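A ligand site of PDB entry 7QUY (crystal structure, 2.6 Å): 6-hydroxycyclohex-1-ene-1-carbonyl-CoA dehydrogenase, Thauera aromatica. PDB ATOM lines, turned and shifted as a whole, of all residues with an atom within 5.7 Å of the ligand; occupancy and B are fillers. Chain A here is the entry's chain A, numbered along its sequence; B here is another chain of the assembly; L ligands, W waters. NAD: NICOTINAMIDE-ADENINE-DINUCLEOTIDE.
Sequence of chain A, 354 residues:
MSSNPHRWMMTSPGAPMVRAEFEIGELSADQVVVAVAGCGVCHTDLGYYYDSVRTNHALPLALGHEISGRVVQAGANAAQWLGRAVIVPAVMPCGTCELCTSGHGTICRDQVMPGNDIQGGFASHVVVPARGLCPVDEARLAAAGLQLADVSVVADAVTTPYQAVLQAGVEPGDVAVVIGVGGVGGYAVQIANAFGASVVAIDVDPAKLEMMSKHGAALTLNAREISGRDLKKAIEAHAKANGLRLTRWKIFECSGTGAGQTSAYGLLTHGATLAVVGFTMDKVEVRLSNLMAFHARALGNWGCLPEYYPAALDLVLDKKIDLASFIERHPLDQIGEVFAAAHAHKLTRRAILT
N of Gly 182 lies within hydrogen-bond range of O3B of the ligand (3.2 Å).
The side-chain carboxylate (OD1) of Asp 203 lies within hydrogen-bond range of an oxygen (O2B) of the ligand (2.5 Å).
N of Phe 279 lies within hydrogen-bond range of O3D of the ligand (2.9 Å).
An oxygen (O7N) of the ligand is in hydrogen-bond range of the backbone NH (N) of Gly 303 (2.6 Å).
O of Val 277 sits at hydrogen-bond distance from N7N of the ligand.
O of Gly 182 lies close to O2N of the ligand, at 2.7 Å.
The backbone carbonyl oxygen (O) of Asn 301 lies within hydrogen-bond range of a nitrogen (N7N) of the ligand (2.8 Å).
The backbone carbonyl oxygen of Phe 279 lies within hydrogen-bond range of an oxygen (O3D) of the ligand, 3.0 Å away.
N of Val 184 lies within hydrogen-bond range of O2N of the ligand (2.8 Å).
The backbone carbonyl oxygen (O) of Ile 202 sits at hydrogen-bond distance from the backbone NH (N) of Gly 180.
N of Gly 260 lies within hydrogen-bond range of OG1 of Thr 257, at 3.1 Å.
The backbone NH (N) of Asp 205 lies within hydrogen-bond range of the side-chain carboxylate (OD1) of Asp 203 (3.2 Å).
O of Gly 303 sits close to OD1 of Asn 301.
OD2 of Asp 203 sits at hydrogen-bond distance from N of Val 181.
The side-chain hydroxyl (OG1) of Thr 160 lies within hydrogen-bond range of the side-chain carboxylate (OD1) of Asp 156.
The backbone NH (N) of Cys 254 sits at hydrogen-bond distance from the backbone carbonyl oxygen (O) of Ile 179.
The side-chain carboxylate of Asp 156 lies close to the side-chain sulfur of Cys 42, 3.6 Å away.
CE1 of His 43 touches O1A of the ligand (3.8 Å).
OD1 of Asp 156 touches C4N of the ligand, at 3.4 Å.
CG2 of Thr 160 touches C4N of the ligand, 3.3 Å away.
CG2 of Ile 179 touches C2A of the ligand, at 3.7 Å.
CA of Gly 180 touches O4B of the ligand (3.4 Å).
Val 181 touches the ligand (N to O3B, 3.8 Å).
Gly 183 touches the ligand.
Val 204 touches the ligand (CG2 to O2B, 3.3 Å).
Lys 208 touches the ligand.
Cys 254 touches the ligand (O to C5D, 3.4 Å).
CA of Ser 255 touches O4B of the ligand, 3.4 Å away.
Gly 256 touches the ligand.
CG2 of Thr 257 touches N7A of the ligand (3.6 Å).
Ala 259 touches the ligand.
Gly 260 touches the ligand (N to N6A, 3.6 Å).
CA of Gly 278 touches O3D of the ligand, 3.6 Å away.
Trp 302 touches the ligand.
Met 292 of chain B touches the ligand.
Hydrophobic or aromatic side chains within 4 Å of the ligand: His 43, Ile 179, Val 184, Val 204, Ala 259, Val 277 and Met 292 of chain B.
25 residues have an atom within 4 Å of the ligand: His 43, Asp 156, Thr 160, Ile 179, Gly 180, Val 181, Gly 182, Gly 183, Val 184, Asp 203, Val 204, Lys 208, Cys 254, Ser 255, Gly 256, Thr 257, Ala 259, Gly 260, Val 277, Gly 278, Phe 279, Asn 301, Trp 302, Gly 303 and Met 292 of chain B.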
ATOM      1  N   CYS A  42       3.373 -17.439  32.775  1.00  0.00           N
ATOM      2  CA  CYS A  42       4.755 -17.854  32.440  1.00  0.00           C
ATOM      3  C   CYS A  42       5.690 -17.746  33.649  1.00  0.00           C
ATOM      4  O   CYS A  42       5.324 -17.073  34.632  1.00  0.00           O
ATOM      5  CB  CYS A  42       5.307 -16.961  31.335  1.00  0.00           C
ATOM      6  SG  CYS A  42       6.964 -17.424  30.771  1.00  0.00           S
ATOM      7  N   HIS A  43       6.857 -18.377  33.558  1.00  0.00           N
ATOM      8  CA  HIS A  43       7.890 -18.358  34.618  1.00  0.00           C
ATOM      9  C   HIS A  43       8.369 -16.909  34.766  1.00  0.00           C
ATOM     10  O   HIS A  43       8.773 -16.533  35.874  1.00  0.00           O
ATOM     11  CB  HIS A  43       9.006 -19.386  34.340  1.00  0.00           C
ATOM     12  CG  HIS A  43       8.653 -20.751  34.829  1.00  0.00           C
ATOM     13  ND1 HIS A  43       9.410 -21.433  35.776  1.00  0.00           N
ATOM     14  CD2 HIS A  43       7.605 -21.565  34.536  1.00  0.00           C
ATOM     15  CE1 HIS A  43       8.848 -22.606  36.020  1.00  0.00           C
ATOM     16  NE2 HIS A  43       7.738 -22.701  35.279  1.00  0.00           N
ATOM     17  N   THR A  44       8.281 -16.115  33.699  1.00  0.00           N
ATOM     18  CA  THR A  44       8.626 -14.673  33.711  1.00  0.00           C
ATOM     19  C   THR A  44       7.668 -13.972  34.691  1.00  0.00           C
ATOM     20  O   THR A  44       8.169 -13.128  35.466  1.00  0.00           O
ATOM     21  CB  THR A  44       8.527 -14.065  32.308  1.00  0.00           C
ATOM     22  OG1 THR A  44       9.290 -14.861  31.409  1.00  0.00           O
ATOM     23  CG2 THR A  44       9.099 -12.673  32.222  1.00  0.00           C
ATOM     24  N   ASP A 156       5.260 -15.922  23.141  1.00  0.00           N
ATOM     25  CA  ASP A 156       6.414 -16.357  23.978  1.00  0.00           C
ATOM     26  C   ASP A 156       6.588 -17.881  23.873  1.00  0.00           C
ATOM     27  O   ASP A 156       7.561 -18.312  23.230  1.00  0.00           O
ATOM     28  CB  ASP A 156       6.293 -15.844  25.411  1.00  0.00           C
ATOM     29  CG  ASP A 156       7.571 -16.045  26.218  1.00  0.00           C
ATOM     30  OD1 ASP A 156       8.639 -16.247  25.607  1.00  0.00           O
ATOM     31  OD2 ASP A 156       7.496 -15.997  27.469  1.00  0.00           O
ATOM     32  N   THR A 160       9.027 -18.149  20.923  1.00  0.00           N
ATOM     33  CA  THR A 160      10.425 -18.066  21.412  1.00  0.00           C
ATOM     34  C   THR A 160      11.213 -19.232  20.807  1.00  0.00           C
ATOM     35  O   THR A 160      12.154 -19.003  20.048  1.00  0.00           O
ATOM     36  CB  THR A 160      10.464 -17.931  22.947  1.00  0.00           C
ATOM     37  OG1 THR A 160      10.062 -16.577  23.196  1.00  0.00           O
ATOM     38  CG2 THR A 160      11.823 -18.221  23.557  1.00  0.00           C
ATOM     39  N   ILE A 179      17.576 -29.891  24.976  1.00  0.00           N
ATOM     40  CA  ILE A 179      17.937 -30.151  26.396  1.00  0.00           C
ATOM     41  C   ILE A 179      17.021 -29.299  27.262  1.00  0.00           C
ATOM     42  O   ILE A 179      17.022 -28.052  27.097  1.00  0.00           O
ATOM     43  CB  ILE A 179      19.424 -29.872  26.636  1.00  0.00           C
ATOM     44  CG1 ILE A 179      20.285 -30.920  25.918  1.00  0.00           C
ATOM     45  CG2 ILE A 179      19.759 -29.813  28.111  1.00  0.00           C
ATOM     46  CD1 ILE A 179      21.616 -30.425  25.484  1.00  0.00           C
ATOM     47  N   GLY A 180      16.267 -29.954  28.147  1.00  0.00           N
ATOM     48  CA  GLY A 180      15.209 -29.329  28.939  1.00  0.00           C
ATOM     49  C   GLY A 180      13.986 -29.143  28.087  1.00  0.00           C
ATOM     50  O   GLY A 180      13.980 -28.265  27.219  1.00  0.00           O
ATOM     51  N   VAL A 181      12.992 -29.988  28.300  1.00  0.00           N
ATOM     52  CA  VAL A 181      11.917 -30.209  27.299  1.00  0.00           C
ATOM     53  C   VAL A 181      10.583 -29.880  27.987  1.00  0.00           C
ATOM     54  O   VAL A 181       9.548 -30.438  27.624  1.00  0.00           O
ATOM     55  CB  VAL A 181      12.057 -31.631  26.733  1.00  0.00           C
ATOM     56  CG1 VAL A 181      11.447 -32.702  27.621  1.00  0.00           C
ATOM     57  CG2 VAL A 181      11.528 -31.704  25.317  1.00  0.00           C
ATOM     58  N   GLY A 182      10.637 -28.949  28.942  1.00  0.00           N
ATOM     59  CA  GLY A 182       9.465 -28.282  29.514  1.00  0.00           C
ATOM     60  C   GLY A 182       9.288 -26.885  28.931  1.00  0.00           C
ATOM     61  O   GLY A 182      10.301 -26.262  28.555  1.00  0.00           O
ATOM     62  N   GLY A 183       8.033 -26.441  28.854  1.00  0.00           N
ATOM     63  CA  GLY A 183       7.625 -25.053  28.582  1.00  0.00           C
ATOM     64  C   GLY A 183       7.971 -24.641  27.166  1.00  0.00           C
ATOM     65  O   GLY A 183       7.233 -25.020  26.230  1.00  0.00           O
ATOM     66  N   VAL A 184       9.080 -23.925  27.040  1.00  0.00           N
ATOM     67  CA  VAL A 184       9.753 -23.542  25.762  1.00  0.00           C
ATOM     68  C   VAL A 184      10.287 -24.808  25.074  1.00  0.00           C
ATOM     69  O   VAL A 184       9.979 -24.991  23.875  1.00  0.00           O
ATOM     70  CB  VAL A 184      10.862 -22.538  26.088  1.00  0.00           C
ATOM     71  CG1 VAL A 184      11.895 -22.432  24.970  1.00  0.00           C
ATOM     72  CG2 VAL A 184      10.269 -21.187  26.431  1.00  0.00           C
ATOM     73  N   GLY A 185      11.057 -25.625  25.795  1.00  0.00           N
ATOM     74  CA  GLY A 185      11.703 -26.840  25.261  1.00  0.00           C
ATOM     75  C   GLY A 185      10.731 -27.774  24.535  1.00  0.00           C
ATOM     76  O   GLY A 185      11.045 -28.249  23.429  1.00  0.00           O
ATOM     77  N   ILE A 202      16.044 -34.452  25.786  1.00  0.00           N
ATOM     78  CA  ILE A 202      16.831 -34.731  27.025  1.00  0.00           C
ATOM     79  C   ILE A 202      16.209 -33.943  28.191  1.00  0.00           C
ATOM     80  O   ILE A 202      15.885 -32.758  28.000  1.00  0.00           O
ATOM     81  CB  ILE A 202      18.318 -34.392  26.825  1.00  0.00           C
ATOM     82  CG1 ILE A 202      18.905 -35.177  25.655  1.00  0.00           C
ATOM     83  CG2 ILE A 202      19.096 -34.598  28.116  1.00  0.00           C
ATOM     84  CD1 ILE A 202      20.377 -34.884  25.375  1.00  0.00           C
ATOM     85  N   ASP A 203      16.043 -34.589  29.342  1.00  0.00           N
ATOM     86  CA  ASP A 203      15.455 -33.967  30.554  1.00  0.00           C
ATOM     87  C   ASP A 203      15.851 -34.783  31.794  1.00  0.00           C
ATOM     88  O   ASP A 203      16.513 -35.832  31.636  1.00  0.00           O
ATOM     89  CB  ASP A 203      13.944 -33.774  30.417  1.00  0.00           C
ATOM     90  CG  ASP A 203      13.413 -32.574  31.174  1.00  0.00           C
ATOM     91  OD1 ASP A 203      13.657 -32.507  32.400  1.00  0.00           O
ATOM     92  OD2 ASP A 203      12.789 -31.675  30.547  1.00  0.00           O
ATOM     93  N   VAL A 204      15.487 -34.274  32.968  1.00  0.00           N
ATOM     94  CA  VAL A 204      15.688 -34.929  34.296  1.00  0.00           C
ATOM     95  C   VAL A 204      14.359 -35.508  34.784  1.00  0.00           C
ATOM     96  O   VAL A 204      14.389 -36.305  35.733  1.00  0.00           O
ATOM     97  CB  VAL A 204      16.289 -33.951  35.325  1.00  0.00           C
ATOM     98  CG1 VAL A 204      17.736 -33.590  34.966  1.00  0.00           C
ATOM     99  CG2 VAL A 204      15.442 -32.699  35.514  1.00  0.00           C
ATOM    100  N   ASP A 205      13.235 -35.141  34.150  1.00  0.00           N
ATOM    101  CA  ASP A 205      11.850 -35.540  34.537  1.00  0.00           C
ATOM    102  C   ASP A 205      11.296 -36.546  33.523  1.00  0.00           C
ATOM    103  O   ASP A 205      10.870 -36.163  32.425  1.00  0.00           O
ATOM    104  CB  ASP A 205      10.964 -34.303  34.700  1.00  0.00           C
ATOM    105  CG  ASP A 205       9.520 -34.589  35.104  1.00  0.00           C
ATOM    106  OD1 ASP A 205       9.183 -35.769  35.315  1.00  0.00           O
ATOM    107  OD2 ASP A 205       8.748 -33.629  35.204  1.00  0.00           O
ATOM    108  N   LYS A 208       7.923 -35.767  31.417  1.00  0.00           N
ATOM    109  CA  LYS A 208       7.988 -34.857  30.250  1.00  0.00           C
ATOM    110  C   LYS A 208       8.612 -35.618  29.087  1.00  0.00           C
ATOM    111  O   LYS A 208       8.159 -35.405  27.941  1.00  0.00           O
ATOM    112  CB  LYS A 208       8.680 -33.517  30.528  1.00  0.00           C
ATOM    113  CG  LYS A 208       9.380 -33.311  31.860  1.00  0.00           C
ATOM    114  CD  LYS A 208       9.550 -31.858  32.225  1.00  0.00           C
ATOM    115  CE  LYS A 208       8.265 -31.065  32.119  1.00  0.00           C
ATOM    116  NZ  LYS A 208       8.287 -29.897  33.027  1.00  0.00           N
ATOM    117  N   ALA A 223      18.865 -37.281  31.702  1.00  0.00           N
ATOM    118  CA  ALA A 223      20.205 -36.709  31.887  1.00  0.00           C
ATOM    119  C   ALA A 223      20.785 -37.164  33.235  1.00  0.00           C
ATOM    120  O   ALA A 223      22.023 -37.104  33.369  1.00  0.00           O
ATOM    121  CB  ALA A 223      20.169 -35.217  31.749  1.00  0.00           C
ATOM    122  N   CYS A 254      17.373 -25.464  26.338  1.00  0.00           N
ATOM    123  CA  CYS A 254      16.083 -24.877  26.778  1.00  0.00           C
ATOM    124  C   CYS A 254      15.846 -25.131  28.275  1.00  0.00           C
ATOM    125  O   CYS A 254      14.699 -24.954  28.730  1.00  0.00           O
ATOM    126  CB  CYS A 254      14.938 -25.432  25.957  1.00  0.00           C
ATOM    127  SG  CYS A 254      15.054 -25.045  24.190  1.00  0.00           S
ATOM    128  N   SER A 255      16.879 -25.536  29.023  1.00  0.00           N
ATOM    129  CA  SER A 255      16.794 -25.829  30.476  1.00  0.00           C
ATOM    130  C   SER A 255      16.941 -24.529  31.290  1.00  0.00           C
ATOM    131  O   SER A 255      16.213 -24.341  32.289  1.00  0.00           O
ATOM    132  CB  SER A 255      17.811 -26.874  30.861  1.00  0.00           C
ATOM    133  OG  SER A 255      19.086 -26.289  31.131  1.00  0.00           O
ATOM    134  N   GLY A 256      17.868 -23.659  30.898  1.00  0.00           N
ATOM    135  CA  GLY A 256      18.209 -22.446  31.660  1.00  0.00           C
ATOM    136  C   GLY A 256      18.967 -22.810  32.913  1.00  0.00           C
ATOM    137  O   GLY A 256      18.761 -22.154  33.966  1.00  0.00           O
ATOM    138  N   THR A 257      19.821 -23.827  32.804  1.00  0.00           N
ATOM    139  CA  THR A 257      20.680 -24.358  33.905  1.00  0.00           C
ATOM    140  C   THR A 257      22.078 -24.629  33.341  1.00  0.00           C
ATOM    141  O   THR A 257      22.180 -25.069  32.185  1.00  0.00           O
ATOM    142  CB  THR A 257      20.092 -25.650  34.490  1.00  0.00           C
ATOM    143  OG1 THR A 257      20.520 -26.708  33.640  1.00  0.00           O
ATOM    144  CG2 THR A 257      18.580 -25.647  34.586  1.00  0.00           C
ATOM    145  N   ALA A 259      24.087 -27.007  33.963  1.00  0.00           N
ATOM    146  CA  ALA A 259      24.217 -28.453  33.642  1.00  0.00           C
ATOM    147  C   ALA A 259      23.779 -28.667  32.186  1.00  0.00           C
ATOM    148  O   ALA A 259      24.571 -29.221  31.403  1.00  0.00           O
ATOM    149  CB  ALA A 259      23.396 -29.260  34.608  1.00  0.00           C
ATOM    150  N   GLY A 260      22.584 -28.195  31.850  1.00  0.00           N
ATOM    151  CA  GLY A 260      22.029 -28.235  30.488  1.00  0.00           C
ATOM    152  C   GLY A 260      22.983 -27.631  29.472  1.00  0.00           C
ATOM    153  O   GLY A 260      23.229 -28.278  28.433  1.00  0.00           O
ATOM    154  N   VAL A 276      21.205 -21.097  22.078  1.00  0.00           N
ATOM    155  CA  VAL A 276      21.138 -20.707  23.531  1.00  0.00           C
ATOM    156  C   VAL A 276      19.813 -19.982  23.782  1.00  0.00           C
ATOM    157  O   VAL A 276      19.704 -18.783  23.439  1.00  0.00           O
ATOM    158  CB  VAL A 276      22.331 -19.825  23.917  1.00  0.00           C
ATOM    159  CG1 VAL A 276      22.260 -19.413  25.375  1.00  0.00           C
ATOM    160  CG2 VAL A 276      23.662 -20.488  23.615  1.00  0.00           C
ATOM    161  N   VAL A 277      18.830 -20.673  24.361  1.00  0.00           N
ATOM    162  CA  VAL A 277      17.446 -20.144  24.566  1.00  0.00           C
ATOM    163  C   VAL A 277      17.218 -19.883  26.062  1.00  0.00           C
ATOM    164  O   VAL A 277      16.665 -18.824  26.416  1.00  0.00           O
ATOM    165  CB  VAL A 277      16.389 -21.089  23.967  1.00  0.00           C
ATOM    166  CG1 VAL A 277      14.989 -20.509  24.109  1.00  0.00           C
ATOM    167  CG2 VAL A 277      16.665 -21.396  22.517  1.00  0.00           C
ATOM    168  N   GLY A 278      17.627 -20.837  26.891  1.00  0.00           N
ATOM    169  CA  GLY A 278      17.569 -20.749  28.357  1.00  0.00           C
ATOM    170  C   GLY A 278      18.521 -19.707  28.892  1.00  0.00           C
ATOM    171  O   GLY A 278      19.610 -19.580  28.335  1.00  0.00           O
ATOM    172  N   PHE A 279      18.114 -19.017  29.958  1.00  0.00           N
ATOM    173  CA  PHE A 279      18.943 -18.028  30.714  1.00  0.00           C
ATOM    174  C   PHE A 279      19.277 -18.583  32.111  1.00  0.00           C
ATOM    175  O   PHE A 279      18.360 -18.976  32.853  1.00  0.00           O
ATOM    176  CB  PHE A 279      18.214 -16.688  30.829  1.00  0.00           C
ATOM    177  CG  PHE A 279      18.973 -15.685  31.661  1.00  0.00           C
ATOM    178  CD1 PHE A 279      20.011 -14.952  31.104  1.00  0.00           C
ATOM    179  CD2 PHE A 279      18.664 -15.507  33.004  1.00  0.00           C
ATOM    180  CE1 PHE A 279      20.724 -14.045  31.876  1.00  0.00           C
ATOM    181  CE2 PHE A 279      19.376 -14.599  33.776  1.00  0.00           C
ATOM    182  CZ  PHE A 279      20.408 -13.879  33.209  1.00  0.00           C
ATOM    183  N   THR A 280      20.562 -18.593  32.450  1.00  0.00           N
ATOM    184  CA  THR A 280      21.066 -18.758  33.841  1.00  0.00           C
ATOM    185  C   THR A 280      22.132 -17.698  34.086  1.00  0.00           C
ATOM    186  O   THR A 280      22.754 -17.247  33.101  1.00  0.00           O
ATOM    187  CB  THR A 280      21.612 -20.169  34.115  1.00  0.00           C
ATOM    188  OG1 THR A 280      21.906 -20.282  35.504  1.00  0.00           O
ATOM    189  CG2 THR A 280      22.868 -20.495  33.344  1.00  0.00           C
ATOM    190  N   ASN A 301      19.134 -16.072  21.373  1.00  0.00           N
ATOM    191  CA  ASN A 301      17.749 -15.787  20.904  1.00  0.00           C
ATOM    192  C   ASN A 301      17.022 -15.040  22.029  1.00  0.00           C
ATOM    193  O   ASN A 301      16.806 -15.637  23.101  1.00  0.00           O
ATOM    194  CB  ASN A 301      17.115 -17.123  20.526  1.00  0.00           C
ATOM    195  CG  ASN A 301      15.632 -16.991  20.316  1.00  0.00           C
ATOM    196  OD1 ASN A 301      15.236 -16.294  19.404  1.00  0.00           O
ATOM    197  ND2 ASN A 301      14.834 -17.616  21.162  1.00  0.00           N
ATOM    198  N   TRP A 302      16.699 -13.760  21.819  1.00  0.00           N
ATOM    199  CA  TRP A 302      15.854 -12.944  22.743  1.00  0.00           C
ATOM    200  C   TRP A 302      14.434 -12.844  22.170  1.00  0.00           C
ATOM    201  O   TRP A 302      14.237 -12.035  21.270  1.00  0.00           O
ATOM    202  CB  TRP A 302      16.441 -11.544  22.973  1.00  0.00           C
ATOM    203  CG  TRP A 302      15.682 -10.692  23.948  1.00  0.00           C
ATOM    204  CD1 TRP A 302      14.775  -9.720  23.663  1.00  0.00           C
ATOM    205  CD2 TRP A 302      15.757 -10.737  25.388  1.00  0.00           C
ATOM    206  NE1 TRP A 302      14.294  -9.145  24.809  1.00  0.00           N
ATOM    207  CE2 TRP A 302      14.864  -9.763  25.881  1.00  0.00           C
ATOM    208  CE3 TRP A 302      16.470 -11.519  26.308  1.00  0.00           C
ATOM    209  CZ2 TRP A 302      14.667  -9.556  27.247  1.00  0.00           C
ATOM    210  CZ3 TRP A 302      16.287 -11.305  27.657  1.00  0.00           C
ATOM    211  CH2 TRP A 302      15.395 -10.342  28.124  1.00  0.00           C
ATOM    212  N   GLY A 303      13.495 -13.649  22.695  1.00  0.00           N
ATOM    213  CA  GLY A 303      12.111 -13.739  22.187  1.00  0.00           C
ATOM    214  C   GLY A 303      12.032 -13.842  20.666  1.00  0.00           C
ATOM    215  O   GLY A 303      12.840 -14.546  20.069  1.00  0.00           O
ATOM    216  N   ARG A 350       0.318 -25.813  30.958  1.00  0.00           N
ATOM    217  CA  ARG A 350       0.525 -24.350  31.039  1.00  0.00           C
ATOM    218  C   ARG A 350      -0.850 -23.723  31.324  1.00  0.00           C
ATOM    219  O   ARG A 350      -1.806 -24.067  30.618  1.00  0.00           O
ATOM    220  CB  ARG A 350       1.155 -23.809  29.741  1.00  0.00           C
ATOM    221  CG  ARG A 350       1.705 -22.392  29.844  1.00  0.00           C
ATOM    222  CD  ARG A 350       2.300 -21.891  28.547  1.00  0.00           C
ATOM    223  NE  ARG A 350       3.157 -20.730  28.727  1.00  0.00           N
ATOM    224  CZ  ARG A 350       4.389 -20.758  29.220  1.00  0.00           C
ATOM    225  NH1 ARG A 350       4.937 -21.910  29.546  1.00  0.00           N
ATOM    226  NH2 ARG A 350       5.082 -19.650  29.331  1.00  0.00           N
ATOM    227  N   MET B 292      21.986 -15.328  24.687  1.00  0.00           N
ATOM    228  CA  MET B 292      20.514 -15.133  24.621  1.00  0.00           C
ATOM    229  C   MET B 292      20.189 -13.706  25.059  1.00  0.00           C
ATOM    230  O   MET B 292      19.368 -13.051  24.362  1.00  0.00           O
ATOM    231  CB  MET B 292      19.728 -16.171  25.438  1.00  0.00           C
ATOM    232  CG  MET B 292      19.548 -15.877  26.914  1.00  0.00           C
ATOM    233  SD  MET B 292      18.183 -14.746  27.289  1.00  0.00           S
ATOM    234  CE  MET B 292      16.812 -15.880  27.374  1.00  0.00           C
HETATM  235  PA  NAD L   1      10.625 -25.003  32.439  1.00  0.00           P
HETATM  236  O1A NAD L   1      10.890 -25.037  33.914  1.00  0.00           O
HETATM  237  O2A NAD L   1       9.233 -25.163  31.923  1.00  0.00           O
HETATM  238  O5B NAD L   1      11.577 -26.074  31.713  1.00  0.00           O
HETATM  239  C5B NAD L   1      12.964 -26.310  32.051  1.00  0.00           C
HETATM  240  C4B NAD L   1      13.244 -27.771  31.782  1.00  0.00           C
HETATM  241  O4B NAD L   1      14.651 -28.052  31.986  1.00  0.00           O
HETATM  242  C3B NAD L   1      12.479 -28.769  32.675  1.00  0.00           C
HETATM  243  O3B NAD L   1      11.790 -29.703  31.862  1.00  0.00           O
HETATM  244  C2B NAD L   1      13.585 -29.355  33.572  1.00  0.00           C
HETATM  245  O2B NAD L   1      13.340 -30.652  34.059  1.00  0.00           O
HETATM  246  C1B NAD L   1      14.731 -29.331  32.573  1.00  0.00           C
HETATM  247  N9A NAD L   1      16.062 -29.491  33.139  1.00  0.00           N
HETATM  248  C8A NAD L   1      16.536 -28.928  34.297  1.00  0.00           C
HETATM  249  N7A NAD L   1      17.789 -29.208  34.517  1.00  0.00           N
HETATM  250  C5A NAD L   1      18.190 -29.974  33.431  1.00  0.00           C
HETATM  251  C6A NAD L   1      19.418 -30.570  33.069  1.00  0.00           C
HETATM  252  N6A NAD L   1      20.513 -30.458  33.810  1.00  0.00           N
HETATM  253  N1A NAD L   1      19.491 -31.255  31.900  1.00  0.00           N
HETATM  254  C2A NAD L   1      18.369 -31.344  31.178  1.00  0.00           C
HETATM  255  N3A NAD L   1      17.153 -30.838  31.425  1.00  0.00           N
HETATM  256  C4A NAD L   1      17.123 -30.147  32.571  1.00  0.00           C
HETATM  257  O3  NAD L   1      11.185 -23.639  31.812  1.00  0.00           O
HETATM  258  PN  NAD L   1      10.715 -22.815  30.510  1.00  0.00           P
HETATM  259  O1N NAD L   1       9.413 -22.161  30.795  1.00  0.00           O
HETATM  260  O2N NAD L   1      10.756 -23.665  29.297  1.00  0.00           O
HETATM  261  O5D NAD L   1      11.938 -21.775  30.445  1.00  0.00           O
HETATM  262  C5D NAD L   1      13.254 -22.392  30.401  1.00  0.00           C
HETATM  263  C4D NAD L   1      14.306 -21.342  30.143  1.00  0.00           C
HETATM  264  O4D NAD L   1      13.904 -20.535  29.009  1.00  0.00           O
HETATM  265  C3D NAD L   1      14.539 -20.351  31.297  1.00  0.00           C
HETATM  266  O3D NAD L   1      15.926 -20.133  31.537  1.00  0.00           O
HETATM  267  C2D NAD L   1      13.792 -19.109  30.796  1.00  0.00           C
HETATM  268  O2D NAD L   1      14.232 -17.950  31.494  1.00  0.00           O
HETATM  269  C1D NAD L   1      14.147 -19.170  29.308  1.00  0.00           C
HETATM  270  N1N NAD L   1      13.311 -18.327  28.408  1.00  0.00           N
HETATM  271  C2N NAD L   1      13.919 -17.426  27.575  1.00  0.00           C
HETATM  272  C3N NAD L   1      13.226 -16.833  26.532  1.00  0.00           C
HETATM  273  C7N NAD L   1      14.020 -16.255  25.380  1.00  0.00           C
HETATM  274  O7N NAD L   1      13.599 -15.253  24.786  1.00  0.00           O
HETATM  275  N7N NAD L   1      15.158 -16.851  25.046  1.00  0.00           N
HETATM  276  C4N NAD L   1      11.846 -16.827  26.602  1.00  0.00           C
HETATM  277  C5N NAD L   1      11.204 -17.642  27.527  1.00  0.00           C
HETATM  278  C6N NAD L   1      11.963 -18.442  28.372  1.00  0.00           C
HETATM  279  O   HOH W   1      12.287 -12.231  25.755  1.00  0.00           O
